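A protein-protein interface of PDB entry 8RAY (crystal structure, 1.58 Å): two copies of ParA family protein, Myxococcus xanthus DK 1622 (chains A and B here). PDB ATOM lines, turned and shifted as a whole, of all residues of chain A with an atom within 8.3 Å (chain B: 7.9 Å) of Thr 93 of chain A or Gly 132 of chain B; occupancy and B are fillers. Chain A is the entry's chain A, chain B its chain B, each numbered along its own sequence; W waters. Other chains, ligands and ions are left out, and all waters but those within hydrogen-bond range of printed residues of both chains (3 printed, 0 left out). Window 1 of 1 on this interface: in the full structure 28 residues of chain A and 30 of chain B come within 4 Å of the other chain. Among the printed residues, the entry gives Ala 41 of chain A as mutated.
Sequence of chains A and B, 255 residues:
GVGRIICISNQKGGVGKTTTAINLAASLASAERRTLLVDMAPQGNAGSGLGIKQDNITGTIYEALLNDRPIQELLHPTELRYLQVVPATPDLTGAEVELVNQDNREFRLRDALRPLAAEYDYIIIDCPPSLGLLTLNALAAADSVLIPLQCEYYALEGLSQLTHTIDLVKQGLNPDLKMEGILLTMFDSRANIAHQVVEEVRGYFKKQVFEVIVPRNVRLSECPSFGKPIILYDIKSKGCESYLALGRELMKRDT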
ATOM      1  N   MET A  40     -13.420 -34.712 -18.452  1.00  0.00           N
ATOM      2  CA  MET A  40     -13.134 -34.301 -17.080  1.00  0.00           C
ATOM      3  C   MET A  40     -11.686 -33.857 -16.877  1.00  0.00           C
ATOM      4  O   MET A  40     -11.298 -33.585 -15.742  1.00  0.00           O
ATOM      5  CB  MET A  40     -13.476 -35.404 -16.064  1.00  0.00           C
ATOM      6  CG  MET A  40     -15.000 -35.637 -16.014  1.00  0.00           C
ATOM      7  SD  MET A  40     -15.749 -34.347 -14.875  1.00  0.00           S
ATOM      8  CE  MET A  40     -15.086 -34.781 -13.269  1.00  0.00           C
ATOM      9  N   ALA A  41     -10.923 -33.716 -17.937  1.00  0.00           N
ATOM     10  CA  ALA A  41      -9.516 -33.312 -17.810  1.00  0.00           C
ATOM     11  C   ALA A  41      -9.411 -31.796 -18.010  1.00  0.00           C
ATOM     12  O   ALA A  41      -9.921 -31.273 -19.007  1.00  0.00           O
ATOM     13  CB  ALA A  41      -8.641 -34.044 -18.857  1.00  0.00           C
ATOM     14  N   PRO A  42      -8.688 -31.070 -17.168  1.00  0.00           N
ATOM     15  CA  PRO A  42      -8.535 -29.630 -17.398  1.00  0.00           C
ATOM     16  C   PRO A  42      -7.880 -29.317 -18.725  1.00  0.00           C
ATOM     17  O   PRO A  42      -8.063 -28.201 -19.230  1.00  0.00           O
ATOM     18  CB  PRO A  42      -7.631 -29.180 -16.218  1.00  0.00           C
ATOM     19  CG  PRO A  42      -7.811 -30.235 -15.155  1.00  0.00           C
ATOM     20  CD  PRO A  42      -7.995 -31.523 -15.938  1.00  0.00           C
ATOM     21  N   GLN A  43      -7.083 -30.251 -19.273  1.00  0.00           N
ATOM     22  CA  GLN A  43      -6.448 -30.026 -20.576  1.00  0.00           C
ATOM     23  C   GLN A  43      -7.456 -29.957 -21.717  1.00  0.00           C
ATOM     24  O   GLN A  43      -7.162 -29.326 -22.736  1.00  0.00           O
ATOM     25  CB  GLN A  43      -5.430 -31.130 -20.834  1.00  0.00           C
ATOM     26  CG  GLN A  43      -4.292 -31.284 -19.796  1.00  0.00           C
ATOM     27  CD  GLN A  43      -4.611 -32.215 -18.604  1.00  0.00           C
ATOM     28  OE1 GLN A  43      -5.763 -32.414 -18.214  1.00  0.00           O
ATOM     29  NE2 GLN A  43      -3.555 -32.723 -17.956  1.00  0.00           N
ATOM     30  N   TYR A  62     -17.585 -27.837 -15.851  1.00  0.00           N
ATOM     31  CA  TYR A  62     -17.406 -27.077 -14.616  1.00  0.00           C
ATOM     32  C   TYR A  62     -18.754 -26.590 -14.061  1.00  0.00           C
ATOM     33  O   TYR A  62     -18.997 -26.659 -12.840  1.00  0.00           O
ATOM     34  CB  TYR A  62     -16.474 -25.890 -14.904  1.00  0.00           C
ATOM     35  CG  TYR A  62     -16.186 -24.984 -13.737  1.00  0.00           C
ATOM     36  CD1 TYR A  62     -17.185 -24.163 -13.194  1.00  0.00           C
ATOM     37  CD2 TYR A  62     -14.910 -24.910 -13.218  1.00  0.00           C
ATOM     38  CE1 TYR A  62     -16.911 -23.329 -12.123  1.00  0.00           C
ATOM     39  CE2 TYR A  62     -14.628 -24.067 -12.137  1.00  0.00           C
ATOM     40  CZ  TYR A  62     -15.638 -23.271 -11.621  1.00  0.00           C
ATOM     41  OH  TYR A  62     -15.287 -22.455 -10.568  1.00  0.00           O
ATOM     42  N   LEU A  66     -19.868 -27.588 -10.090  1.00  0.00           N
ATOM     43  CA  LEU A  66     -19.831 -26.582  -9.037  1.00  0.00           C
ATOM     44  C   LEU A  66     -21.020 -25.619  -9.021  1.00  0.00           C
ATOM     45  O   LEU A  66     -21.308 -25.071  -7.952  1.00  0.00           O
ATOM     46  CB  LEU A  66     -18.565 -25.748  -9.158  1.00  0.00           C
ATOM     47  CG  LEU A  66     -17.300 -26.509  -8.790  1.00  0.00           C
ATOM     48  CD1 LEU A  66     -16.144 -25.595  -8.990  1.00  0.00           C
ATOM     49  CD2 LEU A  66     -17.471 -26.826  -7.297  1.00  0.00           C
ATOM     50  N   THR A  89     -12.684 -27.296 -19.212  1.00  0.00           N
ATOM     51  CA  THR A  89     -12.054 -25.994 -19.093  1.00  0.00           C
ATOM     52  C   THR A  89     -10.782 -26.144 -18.289  1.00  0.00           C
ATOM     53  O   THR A  89     -10.739 -26.978 -17.384  1.00  0.00           O
ATOM     54  CB  THR A  89     -13.011 -25.001 -18.396  1.00  0.00           C
ATOM     55  OG1 THR A  89     -12.344 -23.764 -18.153  1.00  0.00           O
ATOM     56  CG2 THR A  89     -13.657 -25.582 -17.162  1.00  0.00           C
ATOM     57  N   PRO A  90      -9.751 -25.316 -18.525  1.00  0.00           N
ATOM     58  CA  PRO A  90      -8.615 -25.309 -17.604  1.00  0.00           C
ATOM     59  C   PRO A  90      -8.991 -24.931 -16.196  1.00  0.00           C
ATOM     60  O   PRO A  90      -8.233 -25.284 -15.279  1.00  0.00           O
ATOM     61  CB  PRO A  90      -7.636 -24.293 -18.221  1.00  0.00           C
ATOM     62  CG  PRO A  90      -8.515 -23.402 -19.060  1.00  0.00           C
ATOM     63  CD  PRO A  90      -9.633 -24.284 -19.574  1.00  0.00           C
ATOM     64  N   ASP A  91     -10.137 -24.256 -15.998  1.00  0.00           N
ATOM     65  CA  ASP A  91     -10.621 -23.932 -14.654  1.00  0.00           C
ATOM     66  C   ASP A  91     -11.015 -25.173 -13.875  1.00  0.00           C
ATOM     67  O   ASP A  91     -11.292 -25.078 -12.665  1.00  0.00           O
ATOM     68  CB  ASP A  91     -11.813 -22.981 -14.785  1.00  0.00           C
ATOM     69  CG  ASP A  91     -11.417 -21.601 -15.278  1.00  0.00           C
ATOM     70  OD1 ASP A  91     -10.260 -21.344 -15.617  1.00  0.00           O
ATOM     71  OD2 ASP A  91     -12.310 -20.752 -15.396  1.00  0.00           O
ATOM     72  N   LEU A  92     -11.037 -26.352 -14.519  1.00  0.00           N
ATOM     73  CA  LEU A  92     -11.228 -27.549 -13.703  1.00  0.00           C
ATOM     74  C   LEU A  92     -10.087 -27.761 -12.700  1.00  0.00           C
ATOM     75  O   LEU A  92     -10.308 -28.408 -11.674  1.00  0.00           O
ATOM     76  CB  LEU A  92     -11.348 -28.795 -14.576  1.00  0.00           C
ATOM     77  CG  LEU A  92     -12.651 -28.916 -15.356  1.00  0.00           C
ATOM     78  CD1 LEU A  92     -12.631 -30.185 -16.206  1.00  0.00           C
ATOM     79  CD2 LEU A  92     -13.905 -28.913 -14.415  1.00  0.00           C
ATOM     80  N   THR A  93      -8.890 -27.228 -12.952  1.00  0.00           N
ATOM     81  CA  THR A  93      -7.847 -27.299 -11.927  1.00  0.00           C
ATOM     82  C   THR A  93      -8.302 -26.628 -10.624  1.00  0.00           C
ATOM     83  O   THR A  93      -8.198 -27.217  -9.539  1.00  0.00           O
ATOM     84  CB  THR A  93      -6.585 -26.665 -12.477  1.00  0.00           C
ATOM     85  OG1 THR A  93      -6.176 -27.403 -13.645  1.00  0.00           O
ATOM     86  CG2 THR A  93      -5.413 -26.599 -11.392  1.00  0.00           C
ATOM     87  N   GLY A  94      -8.787 -25.386 -10.734  1.00  0.00           N
ATOM     88  CA  GLY A  94      -9.404 -24.711  -9.590  1.00  0.00           C
ATOM     89  C   GLY A  94     -10.613 -25.440  -9.022  1.00  0.00           C
ATOM     90  O   GLY A  94     -10.812 -25.470  -7.810  1.00  0.00           O
ATOM     91  N   ALA A  95     -11.439 -26.037  -9.883  1.00  0.00           N
ATOM     92  CA  ALA A  95     -12.605 -26.752  -9.368  1.00  0.00           C
ATOM     93  C   ALA A  95     -12.194 -27.844  -8.389  1.00  0.00           C
ATOM     94  O   ALA A  95     -12.860 -28.083  -7.381  1.00  0.00           O
ATOM     95  CB  ALA A  95     -13.416 -27.358 -10.516  1.00  0.00           C
ATOM     96  N   GLU A  96     -11.119 -28.556  -8.699  1.00  0.00           N
ATOM     97  CA  GLU A  96     -10.705 -29.662  -7.852  1.00  0.00           C
ATOM     98  C   GLU A  96     -10.326 -29.150  -6.458  1.00  0.00           C
ATOM     99  O   GLU A  96     -10.627 -29.788  -5.436  1.00  0.00           O
ATOM    100  CB  GLU A  96      -9.539 -30.341  -8.553  1.00  0.00           C
ATOM    101  CG  GLU A  96      -9.528 -31.780  -8.381  1.00  0.00           C
ATOM    102  CD  GLU A  96      -8.416 -32.417  -9.190  1.00  0.00           C
ATOM    103  OE1 GLU A  96      -7.399 -31.749  -9.479  1.00  0.00           O
ATOM    104  OE2 GLU A  96      -8.664 -33.531  -9.675  1.00  0.00           O
ATOM    105  N   VAL A  97      -9.727 -27.964  -6.395  1.00  0.00           N
ATOM    106  CA  VAL A  97      -9.391 -27.365  -5.112  1.00  0.00           C
ATOM    107  C   VAL A  97     -10.662 -26.898  -4.394  1.00  0.00           C
ATOM    108  O   VAL A  97     -10.826 -27.097  -3.182  1.00  0.00           O
ATOM    109  CB  VAL A  97      -8.399 -26.217  -5.344  1.00  0.00           C
ATOM    110  CG1 VAL A  97      -8.168 -25.415  -4.036  1.00  0.00           C
ATOM    111  CG2 VAL A  97      -7.079 -26.759  -5.824  1.00  0.00           C
ATOM    112  N   GLU A  98     -11.568 -26.255  -5.122  1.00  0.00           N
ATOM    113  CA  GLU A  98     -12.809 -25.817  -4.512  1.00  0.00           C
ATOM    114  C   GLU A  98     -13.609 -26.999  -3.968  1.00  0.00           C
ATOM    115  O   GLU A  98     -14.210 -26.906  -2.885  1.00  0.00           O
ATOM    116  CB  GLU A  98     -13.626 -25.030  -5.537  1.00  0.00           C
ATOM    117  CG  GLU A  98     -14.967 -24.625  -5.005  1.00  0.00           C
ATOM    118  CD  GLU A  98     -14.798 -23.530  -3.975  1.00  0.00           C
ATOM    119  OE1 GLU A  98     -13.803 -22.780  -4.114  1.00  0.00           O
ATOM    120  OE2 GLU A  98     -15.632 -23.441  -3.038  1.00  0.00           O
ATOM    121  N   LEU A  99     -13.586 -28.145  -4.669  1.00  0.00           N
ATOM    122  CA  LEU A  99     -14.389 -29.267  -4.206  1.00  0.00           C
ATOM    123  C   LEU A  99     -13.899 -29.855  -2.885  1.00  0.00           C
ATOM    124  O   LEU A  99     -14.700 -30.466  -2.161  1.00  0.00           O
ATOM    125  CB  LEU A  99     -14.422 -30.357  -5.262  1.00  0.00           C
ATOM    126  CG  LEU A  99     -15.374 -30.093  -6.430  1.00  0.00           C
ATOM    127  CD1 LEU A  99     -15.052 -31.115  -7.495  1.00  0.00           C
ATOM    128  CD2 LEU A  99     -16.835 -30.146  -5.961  1.00  0.00           C
ATOM    129  N   PRO A 128      -8.324 -37.027 -16.512  1.00  0.00           N
ATOM    130  CA  PRO A 128      -6.967 -36.482 -16.552  1.00  0.00           C
ATOM    131  C   PRO A 128      -5.976 -37.483 -15.988  1.00  0.00           C
ATOM    132  O   PRO A 128      -6.355 -38.469 -15.339  1.00  0.00           O
ATOM    133  CB  PRO A 128      -7.044 -35.230 -15.659  1.00  0.00           C
ATOM    134  CG  PRO A 128      -8.143 -35.567 -14.629  1.00  0.00           C
ATOM    135  CD  PRO A 128      -9.155 -36.391 -15.463  1.00  0.00           C
ATOM    136  N   LEU A 134     -11.133 -34.937  -9.656  1.00  0.00           N
ATOM    137  CA  LEU A 134     -11.787 -35.049 -10.959  1.00  0.00           C
ATOM    138  C   LEU A 134     -11.889 -36.516 -11.377  1.00  0.00           C
ATOM    139  O   LEU A 134     -12.970 -37.003 -11.755  1.00  0.00           O
ATOM    140  CB  LEU A 134     -11.032 -34.225 -12.011  1.00  0.00           C
ATOM    141  CG  LEU A 134     -11.031 -32.709 -11.766  1.00  0.00           C
ATOM    142  CD1 LEU A 134     -10.078 -32.098 -12.777  1.00  0.00           C
ATOM    143  CD2 LEU A 134     -12.444 -32.115 -12.005  1.00  0.00           C
ATOM    144  N   GLN B  11       1.609 -29.596 -18.310  1.00  0.00           N
ATOM    145  CA  GLN B  11       0.414 -30.291 -17.859  1.00  0.00           C
ATOM    146  C   GLN B  11      -0.027 -31.384 -18.841  1.00  0.00           C
ATOM    147  O   GLN B  11      -0.804 -32.250 -18.452  1.00  0.00           O
ATOM    148  CB  GLN B  11      -0.738 -29.296 -17.601  1.00  0.00           C
ATOM    149  CG  GLN B  11      -1.377 -28.737 -18.893  1.00  0.00           C
ATOM    150  CD  GLN B  11      -0.653 -27.517 -19.478  1.00  0.00           C
ATOM    151  OE1 GLN B  11       0.492 -27.223 -19.159  1.00  0.00           O
ATOM    152  NE2 GLN B  11      -1.340 -26.811 -20.376  1.00  0.00           N
ATOM    153  N   MET B  40       8.244 -34.480  -7.732  1.00  0.00           N
ATOM    154  CA  MET B  40       7.003 -33.942  -7.184  1.00  0.00           C
ATOM    155  C   MET B  40       5.791 -34.620  -7.734  1.00  0.00           C
ATOM    156  O   MET B  40       4.667 -34.160  -7.473  1.00  0.00           O
ATOM    157  CB  MET B  40       6.882 -32.425  -7.382  1.00  0.00           C
ATOM    158  CG  MET B  40       7.863 -31.649  -6.541  1.00  0.00           C
ATOM    159  SD  MET B  40       7.182 -31.534  -4.799  1.00  0.00           S
ATOM    160  CE  MET B  40       5.798 -30.439  -5.037  1.00  0.00           C
ATOM    161  N   GLU B  96      -1.729 -33.539  -2.003  1.00  0.00           N
ATOM    162  CA  GLU B  96      -2.211 -32.380  -2.745  1.00  0.00           C
ATOM    163  C   GLU B  96      -3.596 -31.972  -2.238  1.00  0.00           C
ATOM    164  O   GLU B  96      -3.970 -30.787  -2.294  1.00  0.00           O
ATOM    165  CB  GLU B  96      -2.327 -32.686  -4.247  1.00  0.00           C
ATOM    166  CG  GLU B  96      -2.388 -31.368  -5.062  1.00  0.00           C
ATOM    167  CD  GLU B  96      -2.311 -31.625  -6.547  1.00  0.00           C
ATOM    168  OE1 GLU B  96      -3.230 -32.372  -7.009  1.00  0.00           O
ATOM    169  OE2 GLU B  96      -1.345 -31.254  -7.232  1.00  0.00           O
ATOM    170  N   LEU B  99      -2.860 -30.264   1.183  1.00  0.00           N
ATOM    171  CA  LEU B  99      -2.304 -28.920   0.993  1.00  0.00           C
ATOM    172  C   LEU B  99      -3.384 -27.854   0.838  1.00  0.00           C
ATOM    173  O   LEU B  99      -3.126 -26.681   1.135  1.00  0.00           O
ATOM    174  CB  LEU B  99      -1.382 -28.844  -0.212  1.00  0.00           C
ATOM    175  CG  LEU B  99       0.026 -29.380   0.094  1.00  0.00           C
ATOM    176  CD1 LEU B  99       0.843 -29.682  -1.181  1.00  0.00           C
ATOM    177  CD2 LEU B  99       0.787 -28.379   0.976  1.00  0.00           C
ATOM    178  N   GLU B 106       1.232 -22.841  -1.212  1.00  0.00           N
ATOM    179  CA  GLU B 106       1.980 -22.750  -2.470  1.00  0.00           C
ATOM    180  C   GLU B 106       3.486 -22.669  -2.246  1.00  0.00           C
ATOM    181  O   GLU B 106       4.256 -22.855  -3.194  1.00  0.00           O
ATOM    182  CB  GLU B 106       1.560 -21.516  -3.270  1.00  0.00           C
ATOM    183  CG  GLU B 106       0.081 -21.594  -3.840  1.00  0.00           C
ATOM    184  CD  GLU B 106      -0.992 -21.197  -2.830  1.00  0.00           C
ATOM    185  OE1 GLU B 106      -0.669 -20.746  -1.703  1.00  0.00           O
ATOM    186  OE2 GLU B 106      -2.200 -21.389  -3.168  1.00  0.00           O
ATOM    187  N   PRO B 128       4.377 -33.421 -12.029  1.00  0.00           N
ATOM    188  CA  PRO B 128       3.327 -34.259 -12.622  1.00  0.00           C
ATOM    189  C   PRO B 128       2.596 -33.507 -13.732  1.00  0.00           C
ATOM    190  O   PRO B 128       2.712 -32.270 -13.861  1.00  0.00           O
ATOM    191  CB  PRO B 128       2.405 -34.550 -11.435  1.00  0.00           C
ATOM    192  CG  PRO B 128       2.558 -33.293 -10.542  1.00  0.00           C
ATOM    193  CD  PRO B 128       4.005 -32.855 -10.713  1.00  0.00           C
ATOM    194  N   PRO B 129       1.819 -34.219 -14.534  1.00  0.00           N
ATOM    195  CA  PRO B 129       1.001 -33.636 -15.636  1.00  0.00           C
ATOM    196  C   PRO B 129      -0.250 -32.964 -15.080  1.00  0.00           C
ATOM    197  O   PRO B 129      -1.376 -33.466 -15.202  1.00  0.00           O
ATOM    198  CB  PRO B 129       0.649 -34.859 -16.492  1.00  0.00           C
ATOM    199  CG  PRO B 129       0.591 -36.035 -15.469  1.00  0.00           C
ATOM    200  CD  PRO B 129       1.743 -35.693 -14.462  1.00  0.00           C
ATOM    201  N   SER B 130      -0.024 -31.773 -14.540  1.00  0.00           N
ATOM    202  CA  SER B 130      -1.060 -31.020 -13.837  1.00  0.00           C
ATOM    203  C   SER B 130      -0.553 -29.618 -13.551  1.00  0.00           C
ATOM    204  O   SER B 130       0.654 -29.357 -13.550  1.00  0.00           O
ATOM    205  CB  SER B 130      -1.458 -31.678 -12.509  1.00  0.00           C
ATOM    206  OG  SER B 130      -0.301 -31.957 -11.734  1.00  0.00           O
ATOM    207  N   LEU B 131      -1.518 -28.711 -13.296  1.00  0.00           N
ATOM    208  CA  LEU B 131      -1.213 -27.344 -12.861  1.00  0.00           C
ATOM    209  C   LEU B 131      -1.785 -27.098 -11.470  1.00  0.00           C
ATOM    210  O   LEU B 131      -2.050 -25.943 -11.085  1.00  0.00           O
ATOM    211  CB  LEU B 131      -1.758 -26.326 -13.873  1.00  0.00           C
ATOM    212  CG  LEU B 131      -1.133 -26.455 -15.269  1.00  0.00           C
ATOM    213  CD1 LEU B 131      -1.831 -25.480 -16.257  1.00  0.00           C
ATOM    214  CD2 LEU B 131       0.380 -26.293 -15.261  1.00  0.00           C
ATOM    215  N   GLY B 132      -1.978 -28.179 -10.711  1.00  0.00           N
ATOM    216  CA  GLY B 132      -2.474 -28.087  -9.342  1.00  0.00           C
ATOM    217  C   GLY B 132      -1.375 -27.769  -8.345  1.00  0.00           C
ATOM    218  O   GLY B 132      -0.286 -27.308  -8.698  1.00  0.00           O
ATOM    219  N   LEU B 133      -1.683 -27.992  -7.066  1.00  0.00           N
ATOM    220  CA  LEU B 133      -0.824 -27.479  -6.009  1.00  0.00           C
ATOM    221  C   LEU B 133       0.603 -28.092  -6.006  1.00  0.00           C
ATOM    222  O   LEU B 133       1.555 -27.405  -5.635  1.00  0.00           O
ATOM    223  CB  LEU B 133      -1.523 -27.707  -4.665  1.00  0.00           C
ATOM    224  CG  LEU B 133      -2.665 -26.718  -4.446  1.00  0.00           C
ATOM    225  CD1 LEU B 133      -3.384 -27.114  -3.148  1.00  0.00           C
ATOM    226  CD2 LEU B 133      -2.049 -25.292  -4.359  1.00  0.00           C
ATOM    227  N   LEU B 134       0.789 -29.347  -6.462  1.00  0.00           N
ATOM    228  CA  LEU B 134       2.156 -29.879  -6.527  1.00  0.00           C
ATOM    229  C   LEU B 134       2.971 -29.124  -7.572  1.00  0.00           C
ATOM    230  O   LEU B 134       4.083 -28.657  -7.291  1.00  0.00           O
ATOM    231  CB  LEU B 134       2.117 -31.382  -6.840  1.00  0.00           C
ATOM    232  CG  LEU B 134       1.558 -32.259  -5.699  1.00  0.00           C
ATOM    233  CD1 LEU B 134       1.347 -33.717  -6.196  1.00  0.00           C
ATOM    234  CD2 LEU B 134       2.418 -32.204  -4.429  1.00  0.00           C
ATOM    235  N   THR B 135       2.413 -28.977  -8.793  1.00  0.00           N
ATOM    236  CA  THR B 135       3.130 -28.213  -9.808  1.00  0.00           C
ATOM    237  C   THR B 135       3.321 -26.757  -9.411  1.00  0.00           C
ATOM    238  O   THR B 135       4.391 -26.184  -9.688  1.00  0.00           O
ATOM    239  CB  THR B 135       2.411 -28.341 -11.153  1.00  0.00           C
ATOM    240  OG1 THR B 135       2.615 -29.708 -11.531  1.00  0.00           O
ATOM    241  CG2 THR B 135       3.134 -27.496 -12.221  1.00  0.00           C
ATOM    242  N   LEU B 136       2.304 -26.129  -8.795  1.00  0.00           N
ATOM    243  CA  LEU B 136       2.462 -24.733  -8.381  1.00  0.00           C
ATOM    244  C   LEU B 136       3.577 -24.615  -7.348  1.00  0.00           C
ATOM    245  O   LEU B 136       4.351 -23.656  -7.367  1.00  0.00           O
ATOM    246  CB  LEU B 136       1.149 -24.147  -7.803  1.00  0.00           C
ATOM    247  CG  LEU B 136       0.020 -23.996  -8.850  1.00  0.00           C
ATOM    248  CD1 LEU B 136      -1.276 -23.607  -8.198  1.00  0.00           C
ATOM    249  CD2 LEU B 136       0.376 -23.014  -9.955  1.00  0.00           C
ATOM    250  N   ASN B 137       3.679 -25.578  -6.410  1.00  0.00           N
ATOM    251  CA  ASN B 137       4.821 -25.577  -5.482  1.00  0.00           C
ATOM    252  C   ASN B 137       6.148 -25.591  -6.233  1.00  0.00           C
ATOM    253  O   ASN B 137       7.110 -24.901  -5.838  1.00  0.00           O
ATOM    254  CB  ASN B 137       4.750 -26.788  -4.540  1.00  0.00           C
ATOM    255  CG  ASN B 137       4.069 -26.427  -3.206  1.00  0.00           C
ATOM    256  OD1 ASN B 137       4.768 -26.130  -2.224  1.00  0.00           O
ATOM    257  ND2 ASN B 137       2.752 -26.436  -3.164  1.00  0.00           N
ATOM    258  N   ALA B 138       6.242 -26.422  -7.288  1.00  0.00           N
ATOM    259  CA  ALA B 138       7.491 -26.495  -8.031  1.00  0.00           C
ATOM    260  C   ALA B 138       7.778 -25.164  -8.720  1.00  0.00           C
ATOM    261  O   ALA B 138       8.910 -24.667  -8.644  1.00  0.00           O
ATOM    262  CB  ALA B 138       7.430 -27.636  -9.054  1.00  0.00           C
ATOM    263  N   LEU B 139       6.755 -24.564  -9.332  1.00  0.00           N
ATOM    264  CA  LEU B 139       6.949 -23.301 -10.044  1.00  0.00           C
ATOM    265  C   LEU B 139       7.264 -22.184  -9.059  1.00  0.00           C
ATOM    266  O   LEU B 139       8.029 -21.274  -9.381  1.00  0.00           O
ATOM    267  CB  LEU B 139       5.697 -22.918 -10.868  1.00  0.00           C
ATOM    268  CG  LEU B 139       5.500 -23.797 -12.122  1.00  0.00           C
ATOM    269  CD1 LEU B 139       4.044 -23.660 -12.601  1.00  0.00           C
ATOM    270  CD2 LEU B 139       6.471 -23.429 -13.246  1.00  0.00           C
ATOM    271  N   GLN B 161      -1.835 -22.376 -22.568  1.00  0.00           N
ATOM    272  CA  GLN B 161      -2.323 -22.475 -21.194  1.00  0.00           C
ATOM    273  C   GLN B 161      -1.167 -22.614 -20.210  1.00  0.00           C
ATOM    274  O   GLN B 161      -1.192 -22.053 -19.112  1.00  0.00           O
ATOM    275  CB  GLN B 161      -3.281 -23.657 -21.043  1.00  0.00           C
ATOM    276  CG  GLN B 161      -3.764 -23.805 -19.585  1.00  0.00           C
ATOM    277  CD  GLN B 161      -4.609 -22.602 -19.096  1.00  0.00           C
ATOM    278  OE1 GLN B 161      -5.395 -22.051 -19.849  1.00  0.00           O
ATOM    279  NE2 GLN B 161      -4.412 -22.199 -17.844  1.00  0.00           N
ATOM    280  N   THR B 165      -0.261 -19.915 -17.282  1.00  0.00           N
ATOM    281  CA  THR B 165      -0.202 -20.257 -15.876  1.00  0.00           C
ATOM    282  C   THR B 165       1.154 -19.893 -15.295  1.00  0.00           C
ATOM    283  O   THR B 165       1.242 -19.443 -14.140  1.00  0.00           O
ATOM    284  CB  THR B 165      -0.521 -21.743 -15.681  1.00  0.00           C
ATOM    285  OG1 THR B 165      -1.864 -21.980 -16.122  1.00  0.00           O
ATOM    286  CG2 THR B 165      -0.336 -22.134 -14.183  1.00  0.00           C
HETATM  287  O   HOH W   1      -4.339 -29.431 -13.363  1.00  0.00           O
HETATM  288  O   HOH W   2      -5.226 -33.978  -9.285  1.00  0.00           O
HETATM  289  O   HOH W   3      -3.991 -33.272 -14.969  1.00  0.00           O
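O of Pro 129 of chain B touches NE2 of Gln 43 of chain A, at 3.6 Å. Gln 161 of chain B touches Pro 90 of chain A. Leu 131 of chain B touches Thr 93 of chain A. CG2 of Thr 93 of chain A touches N of Gly 132 of chain B, at 3.8 Å.
Printed residues of chain A that touch a printed residue of chain B: Gln 43, Pro 90 and Thr 93. Printed residues of chain B that touch a printed residue of chain A: Gln 11, Pro 129, Leu 131, Gly 132 and Gln 161. Among the printed residues, no Asp or Glu carboxylate lies within 4 Å of a Lys or Arg side-chain nitrogen of the other chain.
Water W3 bridges the backbone carbonyl oxygen (O) of Pro 129 of chain B (2.6 Å) and the side-chain amide nitrogen (NE2) of Gln 43 of chain A (3.1 Å). Water W1 lies within hydrogen-bond range of the side-chain hydroxyl of Thr 93 of chain A (2.8 Å) and the backbone NH of Leu 131 of chain B (2.9 Å). Water W2 bridges the side-chain carboxylate (OE1) of Glu 96 of chain A (3.1 Å) and the side-chain carboxylate (OE1) of Glu 96 of chain B (3.4 Å).
O of Gln 161 of chain B is in hydrogen-bond range of OG1 of Thr 165 of chain B. The side-chain hydroxyl of Thr 93 of chain A lies within hydrogen-bond range of the backbone carbonyl oxygen of Pro 90 of chain A.
5 positions are printed for both chains.
Printed residues of chain B within 4 Å of Thr 93 of chain A: Leu 131 and Gly 132. Of chain A, only Thr 93 (3.8 Å) comes within 4 Å of Gly 132 of chain B. Gly 94 of chain A touches none of the printed residues of chain B. Printed residues of chain A within 4 Å of Pro 129 of chain B: Gln 43. Of the printed residues of chain A, Leu 131 of chain B touches Thr 93. Printed residues of chain A within 4 Å of Gln 11 of chain B: Gln 43 (2.8 Å). Of the printed residues of chain B, Pro 90 of chain A touches Gln 161. Of the printed residues of chain A, Gln 161 of chain B touches Pro 90 (3.5 Å). Leu 99 of chain A touches none of the printed residues of chain B. The nearest printed residue of chain A that does not touch Gln 161 of chain B is Pro 42 of chain A (6.2 Å).
The backbone carbonyl oxygen of Gln 11 of chain B is in hydrogen-bond range of the side-chain amide nitrogen of Gln 43 of chain A.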
